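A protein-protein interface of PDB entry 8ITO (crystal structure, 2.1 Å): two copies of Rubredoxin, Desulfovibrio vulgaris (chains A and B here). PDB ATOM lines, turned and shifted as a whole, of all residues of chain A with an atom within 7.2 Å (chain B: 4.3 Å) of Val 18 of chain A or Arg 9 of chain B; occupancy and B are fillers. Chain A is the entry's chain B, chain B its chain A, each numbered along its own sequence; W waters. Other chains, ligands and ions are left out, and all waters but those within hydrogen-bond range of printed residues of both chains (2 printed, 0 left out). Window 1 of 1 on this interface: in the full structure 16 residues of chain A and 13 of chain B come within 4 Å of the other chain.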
ATOM      1  N   ASP A   6      25.852  27.514  19.876  1.00  0.00           N
ATOM      2  CA  ASP A   6      25.706  26.125  19.458  1.00  0.00           C
ATOM      3  C   ASP A   6      24.381  25.498  19.880  1.00  0.00           C
ATOM      4  O   ASP A   6      24.106  24.359  19.487  1.00  0.00           O
ATOM      5  CB  ASP A   6      26.848  25.277  20.026  1.00  0.00           C
ATOM      6  CG  ASP A   6      28.202  25.846  19.711  1.00  0.00           C
ATOM      7  OD1 ASP A   6      28.539  25.918  18.511  1.00  0.00           O
ATOM      8  OD2 ASP A   6      28.921  26.227  20.666  1.00  0.00           O
ATOM      9  N   MET A   7      23.570  26.200  20.670  1.00  0.00           N
ATOM     10  CA  MET A   7      22.295  25.700  21.151  1.00  0.00           C
ATOM     11  C   MET A   7      21.167  26.274  20.309  1.00  0.00           C
ATOM     12  O   MET A   7      21.205  27.446  19.929  1.00  0.00           O
ATOM     13  CB  MET A   7      22.116  26.055  22.620  1.00  0.00           C
ATOM     14  CG  MET A   7      23.226  25.466  23.481  1.00  0.00           C
ATOM     15  SD  MET A   7      22.813  25.508  25.221  1.00  0.00           S
ATOM     16  CE  MET A   7      23.132  27.248  25.548  1.00  0.00           C
ATOM     17  N   TRP A   8      20.168  25.440  20.010  1.00  0.00           N
ATOM     18  CA  TRP A   8      19.166  25.776  19.012  1.00  0.00           C
ATOM     19  C   TRP A   8      17.779  25.598  19.587  1.00  0.00           C
ATOM     20  O   TRP A   8      17.456  24.531  20.114  1.00  0.00           O
ATOM     21  CB  TRP A   8      19.336  24.918  17.769  1.00  0.00           C
ATOM     22  CG  TRP A   8      20.578  25.272  16.986  1.00  0.00           C
ATOM     23  CD1 TRP A   8      21.882  25.028  17.350  1.00  0.00           C
ATOM     24  CD2 TRP A   8      20.638  25.959  15.717  1.00  0.00           C
ATOM     25  NE1 TRP A   8      22.744  25.502  16.374  1.00  0.00           N
ATOM     26  CE2 TRP A   8      22.006  26.074  15.365  1.00  0.00           C
ATOM     27  CE3 TRP A   8      19.671  26.486  14.851  1.00  0.00           C
ATOM     28  CZ2 TRP A   8      22.427  26.687  14.181  1.00  0.00           C
ATOM     29  CZ3 TRP A   8      20.097  27.094  13.660  1.00  0.00           C
ATOM     30  CH2 TRP A   8      21.461  27.195  13.349  1.00  0.00           C
ATOM     31  N   ARG A   9      16.958  26.632  19.449  1.00  0.00           N
ATOM     32  CA  ARG A   9      15.666  26.713  20.109  1.00  0.00           C
ATOM     33  C   ARG A   9      14.552  26.531  19.094  1.00  0.00           C
ATOM     34  O   ARG A   9      14.527  27.226  18.072  1.00  0.00           O
ATOM     35  CB  ARG A   9      15.516  28.065  20.806  1.00  0.00           C
ATOM     36  CG  ARG A   9      14.223  28.268  21.568  1.00  0.00           C
ATOM     37  CD  ARG A   9      14.428  29.477  22.480  1.00  0.00           C
ATOM     38  NE  ARG A   9      13.441  29.574  23.543  1.00  0.00           N
ATOM     39  CZ  ARG A   9      12.178  29.952  23.378  1.00  0.00           C
ATOM     40  NH1 ARG A   9      11.670  30.187  22.172  1.00  0.00           N
ATOM     41  NH2 ARG A   9      11.403  30.108  24.450  1.00  0.00           N
ATOM     42  N   CYS A  10      13.624  25.628  19.395  1.00  0.00           N
ATOM     43  CA  CYS A  10      12.467  25.420  18.533  1.00  0.00           C
ATOM     44  C   CYS A  10      11.497  26.589  18.697  1.00  0.00           C
ATOM     45  O   CYS A  10      11.006  26.851  19.803  1.00  0.00           O
ATOM     46  CB  CYS A  10      11.779  24.107  18.867  1.00  0.00           C
ATOM     47  SG  CYS A  10      10.322  23.800  17.823  1.00  0.00           S
ATOM     48  N   CYS A  15       6.184  25.940  21.706  1.00  0.00           N
ATOM     49  CA  CYS A  15       7.215  24.948  22.016  1.00  0.00           C
ATOM     50  C   CYS A  15       8.381  25.619  22.755  1.00  0.00           C
ATOM     51  O   CYS A  15       8.191  26.161  23.852  1.00  0.00           O
ATOM     52  CB  CYS A  15       7.688  24.220  20.743  1.00  0.00           C
ATOM     53  SG  CYS A  15       8.754  22.767  21.121  1.00  0.00           S
ATOM     54  N   GLY A  16       9.578  25.632  22.168  1.00  0.00           N
ATOM     55  CA  GLY A  16      10.734  26.211  22.825  1.00  0.00           C
ATOM     56  C   GLY A  16      11.723  25.199  23.359  1.00  0.00           C
ATOM     57  O   GLY A  16      12.600  25.566  24.154  1.00  0.00           O
ATOM     58  N   TYR A  17      11.594  23.936  22.966  1.00  0.00           N
ATOM     59  CA  TYR A  17      12.630  22.950  23.199  1.00  0.00           C
ATOM     60  C   TYR A  17      13.970  23.433  22.648  1.00  0.00           C
ATOM     61  O   TYR A  17      14.047  23.995  21.546  1.00  0.00           O
ATOM     62  CB  TYR A  17      12.237  21.645  22.515  1.00  0.00           C
ATOM     63  CG  TYR A  17      13.325  20.604  22.526  1.00  0.00           C
ATOM     64  CD1 TYR A  17      14.327  20.574  21.531  1.00  0.00           C
ATOM     65  CD2 TYR A  17      13.362  19.652  23.530  1.00  0.00           C
ATOM     66  CE1 TYR A  17      15.332  19.598  21.556  1.00  0.00           C
ATOM     67  CE2 TYR A  17      14.344  18.675  23.567  1.00  0.00           C
ATOM     68  CZ  TYR A  17      15.322  18.645  22.595  1.00  0.00           C
ATOM     69  OH  TYR A  17      16.269  17.648  22.671  1.00  0.00           O
ATOM     70  N   VAL A  18      15.034  23.186  23.401  1.00  0.00           N
ATOM     71  CA  VAL A  18      16.389  23.538  22.979  1.00  0.00           C
ATOM     72  C   VAL A  18      17.186  22.262  22.711  1.00  0.00           C
ATOM     73  O   VAL A  18      17.261  21.348  23.561  1.00  0.00           O
ATOM     74  CB  VAL A  18      17.088  24.432  24.013  1.00  0.00           C
ATOM     75  CG1 VAL A  18      18.522  24.643  23.640  1.00  0.00           C
ATOM     76  CG2 VAL A  18      16.359  25.780  24.081  1.00  0.00           C
ATOM     77  N   TYR A  19      17.757  22.190  21.509  1.00  0.00           N
ATOM     78  CA  TYR A  19      18.764  21.183  21.220  1.00  0.00           C
ATOM     79  C   TYR A  19      20.096  21.672  21.760  1.00  0.00           C
ATOM     80  O   TYR A  19      20.629  22.686  21.296  1.00  0.00           O
ATOM     81  CB  TYR A  19      18.883  20.892  19.723  1.00  0.00           C
ATOM     82  CG  TYR A  19      19.913  19.807  19.494  1.00  0.00           C
ATOM     83  CD1 TYR A  19      19.607  18.479  19.773  1.00  0.00           C
ATOM     84  CD2 TYR A  19      21.210  20.114  19.084  1.00  0.00           C
ATOM     85  CE1 TYR A  19      20.536  17.481  19.603  1.00  0.00           C
ATOM     86  CE2 TYR A  19      22.157  19.122  18.918  1.00  0.00           C
ATOM     87  CZ  TYR A  19      21.809  17.806  19.173  1.00  0.00           C
ATOM     88  OH  TYR A  19      22.719  16.795  19.020  1.00  0.00           O
ATOM     89  N   ASP A  20      20.619  20.955  22.743  1.00  0.00           N
ATOM     90  CA  ASP A  20      21.911  21.235  23.358  1.00  0.00           C
ATOM     91  C   ASP A  20      22.900  20.189  22.864  1.00  0.00           C
ATOM     92  O   ASP A  20      22.797  19.020  23.268  1.00  0.00           O
ATOM     93  CB  ASP A  20      21.778  21.179  24.877  1.00  0.00           C
ATOM     94  CG  ASP A  20      23.044  21.582  25.600  1.00  0.00           C
ATOM     95  OD1 ASP A  20      24.150  21.391  25.051  1.00  0.00           O
ATOM     96  OD2 ASP A  20      22.922  22.084  26.740  1.00  0.00           O
ATOM     97  N   PRO A  21      23.852  20.529  21.993  1.00  0.00           N
ATOM     98  CA  PRO A  21      24.687  19.474  21.396  1.00  0.00           C
ATOM     99  C   PRO A  21      25.416  18.619  22.426  1.00  0.00           C
ATOM    100  O   PRO A  21      25.732  17.464  22.127  1.00  0.00           O
ATOM    101  CB  PRO A  21      25.662  20.251  20.494  1.00  0.00           C
ATOM    102  CG  PRO A  21      25.632  21.682  21.008  1.00  0.00           C
ATOM    103  CD  PRO A  21      24.216  21.871  21.501  1.00  0.00           C
ATOM    104  N   ARG A  23      24.109  17.468  25.205  1.00  0.00           N
ATOM    105  CA  ARG A  23      23.122  16.474  25.620  1.00  0.00           C
ATOM    106  C   ARG A  23      22.892  15.421  24.549  1.00  0.00           C
ATOM    107  O   ARG A  23      22.638  14.257  24.865  1.00  0.00           O
ATOM    108  CB  ARG A  23      21.778  17.151  25.902  1.00  0.00           C
ATOM    109  CG  ARG A  23      21.622  17.880  27.206  1.00  0.00           C
ATOM    110  CD  ARG A  23      20.133  18.246  27.369  1.00  0.00           C
ATOM    111  NE  ARG A  23      19.316  17.118  27.818  1.00  0.00           N
ATOM    112  CZ  ARG A  23      18.492  16.410  27.050  1.00  0.00           C
ATOM    113  NH1 ARG A  23      18.363  16.658  25.754  1.00  0.00           N
ATOM    114  NH2 ARG A  23      17.765  15.434  27.601  1.00  0.00           N
ATOM    115  N   GLY A  24      22.931  15.811  23.280  1.00  0.00           N
ATOM    116  CA  GLY A  24      22.320  14.934  22.301  1.00  0.00           C
ATOM    117  C   GLY A  24      20.805  14.996  22.424  1.00  0.00           C
ATOM    118  O   GLY A  24      20.227  15.983  22.907  1.00  0.00           O
ATOM    119  N   ARG A  27      15.267  10.909  22.741  1.00  0.00           N
ATOM    120  CA  ARG A  27      14.111  10.535  21.929  1.00  0.00           C
ATOM    121  C   ARG A  27      14.465  10.436  20.445  1.00  0.00           C
ATOM    122  O   ARG A  27      13.992   9.531  19.756  1.00  0.00           O
ATOM    123  CB  ARG A  27      12.968  11.529  22.147  1.00  0.00           C
ATOM    124  CG  ARG A  27      12.178  11.284  23.437  1.00  0.00           C
ATOM    125  CD  ARG A  27      11.289  12.475  23.764  1.00  0.00           C
ATOM    126  NE  ARG A  27      12.046  13.646  24.194  1.00  0.00           N
ATOM    127  CZ  ARG A  27      11.494  14.793  24.578  1.00  0.00           C
ATOM    128  NH1 ARG A  27      10.178  14.990  24.515  1.00  0.00           N
ATOM    129  NH2 ARG A  27      12.277  15.764  25.054  1.00  0.00           N
ATOM    130  N   TRP A  43      15.639  14.580  11.195  1.00  0.00           N
ATOM    131  CA  TRP A  43      15.532  14.849  12.628  1.00  0.00           C
ATOM    132  C   TRP A  43      14.481  15.922  12.893  1.00  0.00           C
ATOM    133  O   TRP A  43      14.424  16.942  12.200  1.00  0.00           O
ATOM    134  CB  TRP A  43      16.884  15.302  13.198  1.00  0.00           C
ATOM    135  CG  TRP A  43      16.844  15.568  14.672  1.00  0.00           C
ATOM    136  CD1 TRP A  43      17.184  14.697  15.669  1.00  0.00           C
ATOM    137  CD2 TRP A  43      16.427  16.782  15.321  1.00  0.00           C
ATOM    138  NE1 TRP A  43      17.016  15.297  16.900  1.00  0.00           N
ATOM    139  CE2 TRP A  43      16.537  16.570  16.712  1.00  0.00           C
ATOM    140  CE3 TRP A  43      15.957  18.025  14.858  1.00  0.00           C
ATOM    141  CZ2 TRP A  43      16.203  17.548  17.645  1.00  0.00           C
ATOM    142  CZ3 TRP A  43      15.640  18.996  15.778  1.00  0.00           C
ATOM    143  CH2 TRP A  43      15.759  18.755  17.161  1.00  0.00           C
ATOM    144  N   CYS A  45      12.046  18.080  16.100  1.00  0.00           N
ATOM    145  CA  CYS A  45      11.824  18.415  17.496  1.00  0.00           C
ATOM    146  C   CYS A  45      11.150  17.255  18.218  1.00  0.00           C
ATOM    147  O   CYS A  45      10.090  16.782  17.775  1.00  0.00           O
ATOM    148  CB  CYS A  45      10.955  19.664  17.630  1.00  0.00           C
ATOM    149  SG  CYS A  45      10.662  20.138  19.352  1.00  0.00           S
ATOM    150  N   PRO A  46      11.712  16.778  19.330  1.00  0.00           N
ATOM    151  CA  PRO A  46      11.068  15.659  20.042  1.00  0.00           C
ATOM    152  C   PRO A  46       9.747  16.049  20.682  1.00  0.00           C
ATOM    153  O   PRO A  46       8.937  15.160  20.986  1.00  0.00           O
ATOM    154  CB  PRO A  46      12.105  15.243  21.100  1.00  0.00           C
ATOM    155  CG  PRO A  46      13.161  16.312  21.118  1.00  0.00           C
ATOM    156  CD  PRO A  46      12.911  17.302  20.010  1.00  0.00           C
ATOM    157  N   ILE A  47       9.483  17.337  20.871  1.00  0.00           N
ATOM    158  CA  ILE A  47       8.224  17.734  21.474  1.00  0.00           C
ATOM    159  C   ILE A  47       7.156  17.959  20.422  1.00  0.00           C
ATOM    160  O   ILE A  47       6.060  17.400  20.517  1.00  0.00           O
ATOM    161  CB  ILE A  47       8.388  18.982  22.356  1.00  0.00           C
ATOM    162  CG1 ILE A  47       9.338  18.707  23.519  1.00  0.00           C
ATOM    163  CG2 ILE A  47       7.028  19.352  22.936  1.00  0.00           C
ATOM    164  CD1 ILE A  47       9.414  19.864  24.541  1.00  0.00           C
ATOM    165  N   PHE A  55      14.054  26.049  13.972  1.00  0.00           N
ATOM    166  CA  PHE A  55      14.928  26.360  15.101  1.00  0.00           C
ATOM    167  C   PHE A  55      15.774  27.598  14.816  1.00  0.00           C
ATOM    168  O   PHE A  55      16.006  27.954  13.661  1.00  0.00           O
ATOM    169  CB  PHE A  55      15.867  25.181  15.401  1.00  0.00           C
ATOM    170  CG  PHE A  55      15.202  24.015  16.098  1.00  0.00           C
ATOM    171  CD1 PHE A  55      14.174  23.315  15.487  1.00  0.00           C
ATOM    172  CD2 PHE A  55      15.623  23.615  17.361  1.00  0.00           C
ATOM    173  CE1 PHE A  55      13.570  22.241  16.127  1.00  0.00           C
ATOM    174  CE2 PHE A  55      15.037  22.537  18.000  1.00  0.00           C
ATOM    175  CZ  PHE A  55      13.989  21.860  17.383  1.00  0.00           C
ATOM    176  N   ARG A  56      16.282  28.229  15.869  1.00  0.00           N
ATOM    177  CA  ARG A  56      17.317  29.238  15.674  1.00  0.00           C
ATOM    178  C   ARG A  56      18.327  29.163  16.807  1.00  0.00           C
ATOM    179  O   ARG A  56      17.992  28.727  17.911  1.00  0.00           O
ATOM    180  CB  ARG A  56      16.773  30.673  15.611  1.00  0.00           C
ATOM    181  CG  ARG A  56      15.651  30.981  16.542  1.00  0.00           C
ATOM    182  CD  ARG A  56      15.545  32.481  16.785  1.00  0.00           C
ATOM    183  NE  ARG A  56      14.733  32.776  17.960  1.00  0.00           N
ATOM    184  CZ  ARG A  56      15.150  32.730  19.220  1.00  0.00           C
ATOM    185  NH1 ARG A  56      16.430  32.558  19.528  1.00  0.00           N
ATOM    186  NH2 ARG A  56      14.257  32.858  20.201  1.00  0.00           N
ATOM    187  N   LEU A  58      20.642  30.243  19.969  1.00  0.00           N
ATOM    188  CA  LEU A  58      20.464  31.156  21.095  1.00  0.00           C
ATOM    189  C   LEU A  58      21.323  32.422  20.980  1.00  0.00           C
ATOM    190  O   LEU A  58      21.043  33.405  21.671  1.00  0.00           O
ATOM    191  CB  LEU A  58      20.779  30.439  22.404  1.00  0.00           C
ATOM    192  CG  LEU A  58      19.768  29.420  22.929  1.00  0.00           C
ATOM    193  CD1 LEU A  58      20.005  29.210  24.417  1.00  0.00           C
ATOM    194  CD2 LEU A  58      18.364  29.897  22.678  1.00  0.00           C
ATOM    195  N   TRP B   8      19.176  27.855  32.634  1.00  0.00           N
ATOM    196  CA  TRP B   8      18.657  26.713  33.381  1.00  0.00           C
ATOM    197  C   TRP B   8      17.749  25.905  32.470  1.00  0.00           C
ATOM    198  O   TRP B   8      16.857  26.471  31.829  1.00  0.00           O
ATOM    199  CB  TRP B   8      17.865  27.149  34.616  1.00  0.00           C
ATOM    200  CG  TRP B   8      18.667  27.798  35.675  1.00  0.00           C
ATOM    201  CD1 TRP B   8      19.298  29.007  35.610  1.00  0.00           C
ATOM    202  CD2 TRP B   8      18.931  27.274  36.979  1.00  0.00           C
ATOM    203  NE1 TRP B   8      19.937  29.267  36.798  1.00  0.00           N
ATOM    204  CE2 TRP B   8      19.728  28.213  37.652  1.00  0.00           C
ATOM    205  CE3 TRP B   8      18.569  26.096  37.641  1.00  0.00           C
ATOM    206  CZ2 TRP B   8      20.168  28.017  38.956  1.00  0.00           C
ATOM    207  CZ3 TRP B   8      18.999  25.909  38.932  1.00  0.00           C
ATOM    208  CH2 TRP B   8      19.799  26.865  39.577  1.00  0.00           C
ATOM    209  N   ARG B   9      17.966  24.593  32.431  1.00  0.00           N
ATOM    210  CA  ARG B   9      17.203  23.686  31.591  1.00  0.00           C
ATOM    211  C   ARG B   9      16.230  22.869  32.426  1.00  0.00           C
ATOM    212  O   ARG B   9      16.610  22.296  33.459  1.00  0.00           O
ATOM    213  CB  ARG B   9      18.128  22.746  30.829  1.00  0.00           C
ATOM    214  CG  ARG B   9      17.436  22.050  29.676  1.00  0.00           C
ATOM    215  CD  ARG B   9      18.342  20.971  29.088  1.00  0.00           C
ATOM    216  NE  ARG B   9      17.651  20.177  28.085  1.00  0.00           N
ATOM    217  CZ  ARG B   9      17.637  20.476  26.793  1.00  0.00           C
ATOM    218  NH1 ARG B   9      18.303  21.518  26.318  1.00  0.00           N
ATOM    219  NH2 ARG B   9      16.950  19.705  25.957  1.00  0.00           N
ATOM    220  N   CYS B  10      14.985  22.802  31.964  1.00  0.00           N
ATOM    221  CA  CYS B  10      13.983  21.948  32.593  1.00  0.00           C
ATOM    222  C   CYS B  10      14.331  20.481  32.406  1.00  0.00           C
ATOM    223  O   CYS B  10      14.587  20.032  31.286  1.00  0.00           O
ATOM    224  CB  CYS B  10      12.605  22.213  32.007  1.00  0.00           C
ATOM    225  SG  CYS B  10      11.341  21.254  32.830  1.00  0.00           S
ATOM    226  N   GLN B  11      14.296  19.721  33.492  1.00  0.00           N
ATOM    227  CA  GLN B  11      14.810  18.357  33.461  1.00  0.00           C
ATOM    228  C   GLN B  11      13.731  17.289  33.314  1.00  0.00           C
ATOM    229  O   GLN B  11      14.081  16.110  33.226  1.00  0.00           O
ATOM    230  CB  GLN B  11      15.651  18.072  34.718  1.00  0.00           C
ATOM    231  CG  GLN B  11      16.982  18.833  34.788  1.00  0.00           C
ATOM    232  CD  GLN B  11      17.874  18.617  33.567  1.00  0.00           C
ATOM    233  OE1 GLN B  11      18.296  17.498  33.275  1.00  0.00           O
ATOM    234  NE2 GLN B  11      18.165  19.693  32.847  1.00  0.00           N
ATOM    235  N   GLY B  16      12.550  20.165  28.020  1.00  0.00           N
ATOM    236  CA  GLY B  16      13.808  20.619  27.453  1.00  0.00           C
ATOM    237  C   GLY B  16      13.808  22.111  27.183  1.00  0.00           C
ATOM    238  O   GLY B  16      14.649  22.624  26.442  1.00  0.00           O
ATOM    239  N   TYR B  17      12.838  22.807  27.762  1.00  0.00           N
ATOM    240  CA  TYR B  17      12.876  24.256  27.807  1.00  0.00           C
ATOM    241  C   TYR B  17      14.113  24.716  28.559  1.00  0.00           C
ATOM    242  O   TYR B  17      14.511  24.100  29.552  1.00  0.00           O
ATOM    243  CB  TYR B  17      11.644  24.792  28.523  1.00  0.00           C
ATOM    244  CG  TYR B  17      11.613  26.302  28.635  1.00  0.00           C
ATOM    245  CD1 TYR B  17      11.205  27.092  27.560  1.00  0.00           C
ATOM    246  CD2 TYR B  17      11.979  26.942  29.830  1.00  0.00           C
ATOM    247  CE1 TYR B  17      11.143  28.493  27.666  1.00  0.00           C
ATOM    248  CE2 TYR B  17      11.924  28.343  29.951  1.00  0.00           C
ATOM    249  CZ  TYR B  17      11.508  29.107  28.861  1.00  0.00           C
ATOM    250  OH  TYR B  17      11.464  30.479  28.973  1.00  0.00           O
ATOM    251  N   VAL B  18      14.718  25.798  28.072  1.00  0.00           N
ATOM    252  CA  VAL B  18      15.837  26.458  28.732  1.00  0.00           C
ATOM    253  C   VAL B  18      15.396  27.867  29.091  1.00  0.00           C
ATOM    254  O   VAL B  18      15.043  28.645  28.201  1.00  0.00           O
ATOM    255  CB  VAL B  18      17.091  26.503  27.839  1.00  0.00           C
ATOM    256  CG1 VAL B  18      18.180  27.279  28.547  1.00  0.00           C
ATOM    257  CG2 VAL B  18      17.578  25.096  27.493  1.00  0.00           C
ATOM    258  N   CYS B  54      12.633  21.555  39.156  1.00  0.00           N
ATOM    259  CA  CYS B  54      12.945  20.642  38.072  1.00  0.00           C
ATOM    260  C   CYS B  54      14.010  21.187  37.125  1.00  0.00           C
ATOM    261  O   CYS B  54      14.274  20.564  36.093  1.00  0.00           O
ATOM    262  CB  CYS B  54      11.672  20.306  37.296  1.00  0.00           C
ATOM    263  SG  CYS B  54      10.427  19.356  38.251  1.00  0.00           S
ATOM    264  N   PHE B  55      14.636  22.317  37.451  1.00  0.00           N
ATOM    265  CA  PHE B  55      15.598  22.961  36.564  1.00  0.00           C
ATOM    266  C   PHE B  55      17.029  22.828  37.087  1.00  0.00           C
ATOM    267  O   PHE B  55      17.272  22.704  38.286  1.00  0.00           O
ATOM    268  CB  PHE B  55      15.253  24.439  36.386  1.00  0.00           C
ATOM    269  CG  PHE B  55      14.094  24.678  35.467  1.00  0.00           C
ATOM    270  CD1 PHE B  55      12.805  24.430  35.886  1.00  0.00           C
ATOM    271  CD2 PHE B  55      14.303  25.145  34.172  1.00  0.00           C
ATOM    272  CE1 PHE B  55      11.732  24.646  35.038  1.00  0.00           C
ATOM    273  CE2 PHE B  55      13.239  25.351  33.318  1.00  0.00           C
ATOM    274  CZ  PHE B  55      11.949  25.102  33.752  1.00  0.00           C
ATOM    275  N   ARG B  56      17.980  22.917  36.163  1.00  0.00           N
ATOM    276  CA  ARG B  56      19.397  22.679  36.396  1.00  0.00           C
ATOM    277  C   ARG B  56      20.168  23.705  35.582  1.00  0.00           C
ATOM    278  O   ARG B  56      19.833  23.908  34.407  1.00  0.00           O
ATOM    279  CB  ARG B  56      19.778  21.276  35.916  1.00  0.00           C
ATOM    280  CG  ARG B  56      20.823  20.577  36.683  1.00  0.00           C
ATOM    281  CD  ARG B  56      20.789  19.091  36.364  1.00  0.00           C
ATOM    282  NE  ARG B  56      21.520  18.732  35.152  1.00  0.00           N
ATOM    283  CZ  ARG B  56      21.805  17.479  34.810  1.00  0.00           C
ATOM    284  NH1 ARG B  56      21.448  16.456  35.572  1.00  0.00           N
ATOM    285  NH2 ARG B  56      22.477  17.246  33.684  1.00  0.00           N
ATOM    286  N   LEU B  58      23.064  25.134  33.119  1.00  0.00           N
ATOM    287  CA  LEU B  58      23.546  24.411  31.944  1.00  0.00           C
ATOM    288  C   LEU B  58      24.955  23.870  32.137  1.00  0.00           C
ATOM    289  O   LEU B  58      25.291  22.819  31.583  1.00  0.00           O
ATOM    290  CB  LEU B  58      23.512  25.308  30.708  1.00  0.00           C
ATOM    291  CG  LEU B  58      22.133  25.633  30.151  1.00  0.00           C
ATOM    292  CD1 LEU B  58      22.266  26.135  28.736  1.00  0.00           C
ATOM    293  CD2 LEU B  58      21.256  24.412  30.215  1.00  0.00           C
HETATM  294  O   HOH W   1      13.694  27.696  25.365  1.00  0.00           O
HETATM  295  O   HOH W   2      15.338  17.739  27.149  1.00  0.00           O
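The backbone NH (N) of Val 18 of chain A sits at hydrogen-bond distance from the backbone carbonyl oxygen (O) of Gly 16 of chain B (3.1 Å). NH1 of Arg 23 of chain A lies close to NH2 of Arg 9 of chain B. The guanidinium group (NH2) of Arg 9 of chain B sits at hydrogen-bond distance from the backbone carbonyl oxygen (O) of Val 18 of chain A (2.9 Å).
The backbone NH of Cys 10 of chain A sits at hydrogen-bond distance from the backbone carbonyl oxygen of Tyr 17 of chain A (2.7 Å). The backbone carbonyl oxygen (O) of Cys 10 of chain A is in hydrogen-bond range of the backbone NH (N) of Gly 16 of chain A (3.0 Å). The backbone carbonyl oxygen of Arg 56 of chain B sits at hydrogen-bond distance from the backbone NH of Arg 9 of chain B. The backbone carbonyl oxygen (O) of Met 7 of chain A sits at hydrogen-bond distance from the backbone NH (N) of Leu 58 of chain A (2.9 Å). N of Cys 10 of chain B is in hydrogen-bond range of O of Tyr 17 of chain B, 2.8 Å away. N of Arg 9 of chain A sits at hydrogen-bond distance from O of Arg 56 of chain A (2.8 Å).
Among the printed residues, pairs that only touch across the chains: Met 7 of chain A with Leu 58 of chain B (3.5 Å), Val 18 of chain A with Val 18 of chain B (3.6 Å), Arg 9 of chain A with Tyr 17 of chain B (3.6 Å), Tyr 17 of chain A with Arg 9 of chain B (3.7 Å), Asp 20 of chain A with Arg 9 of chain B (3.8 Å), Tyr 17 of chain A with Gly 16 of chain B (3.8 Å) and Gly 16 of chain A with Tyr 17 of chain B (3.9 Å).
Val 18 of chain A touches three residues of chain B. Printed residues of chain A within 4 Å of Gly 16 of chain B: Tyr 17 (3.8 Å) and Val 18 (3.1 Å). Printed residues of chain A within 4 Å of Val 18 of chain B: Val 18 (3.6 Å). The nearest printed residue of chain B that does not touch Val 18 of chain A is Tyr 17 of chain B (4.9 Å). The nearest printed residue of chain B that does not touch Met 7 of chain A is Val 18 of chain B (5.7 Å).
Of the 11 printed residues of chain B, 5 touch a printed residue of chain A. Along chain B the printed residues that touch a printed residue of chain A span positions 9 to 58. Among the printed residues, no Asp or Glu carboxylate lies within 4 Å of a Lys or Arg side-chain nitrogen of the other chain.
Gly 16 of chain A touches Tyr 17 of chain B, and with the chains exchanged Tyr 17 of chain A touches Gly 16 of chain B. Val 18 of chain A touches Arg 9 of chain B, but with the chains exchanged Arg 9 of chain A does not touch Val 18 of chain B (5.0 Å). Val 18 of chain A touches Gly 16 of chain B, but with the chains exchanged Gly 16 of chain A does not touch Val 18 of chain B (4.5 Å). Val 18 of chain A touches its own counterpart, Val 18 of chain B. Of the 10 pairs that touch across the chains among the printed residues, 5 have their exchanged pair printed and touching as well.
Water W1 lies within hydrogen-bond range of NE of Arg 9 of chain A (2.6 Å), O of Gly 16 of chain A (2.7 Å) and O of Val 18 of chain B (3.3 Å). Water W2 bridges NH2 of Arg 9 of chain B (2.8 Å) and NH2 of Arg 23 of chain A (3.4 Å).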
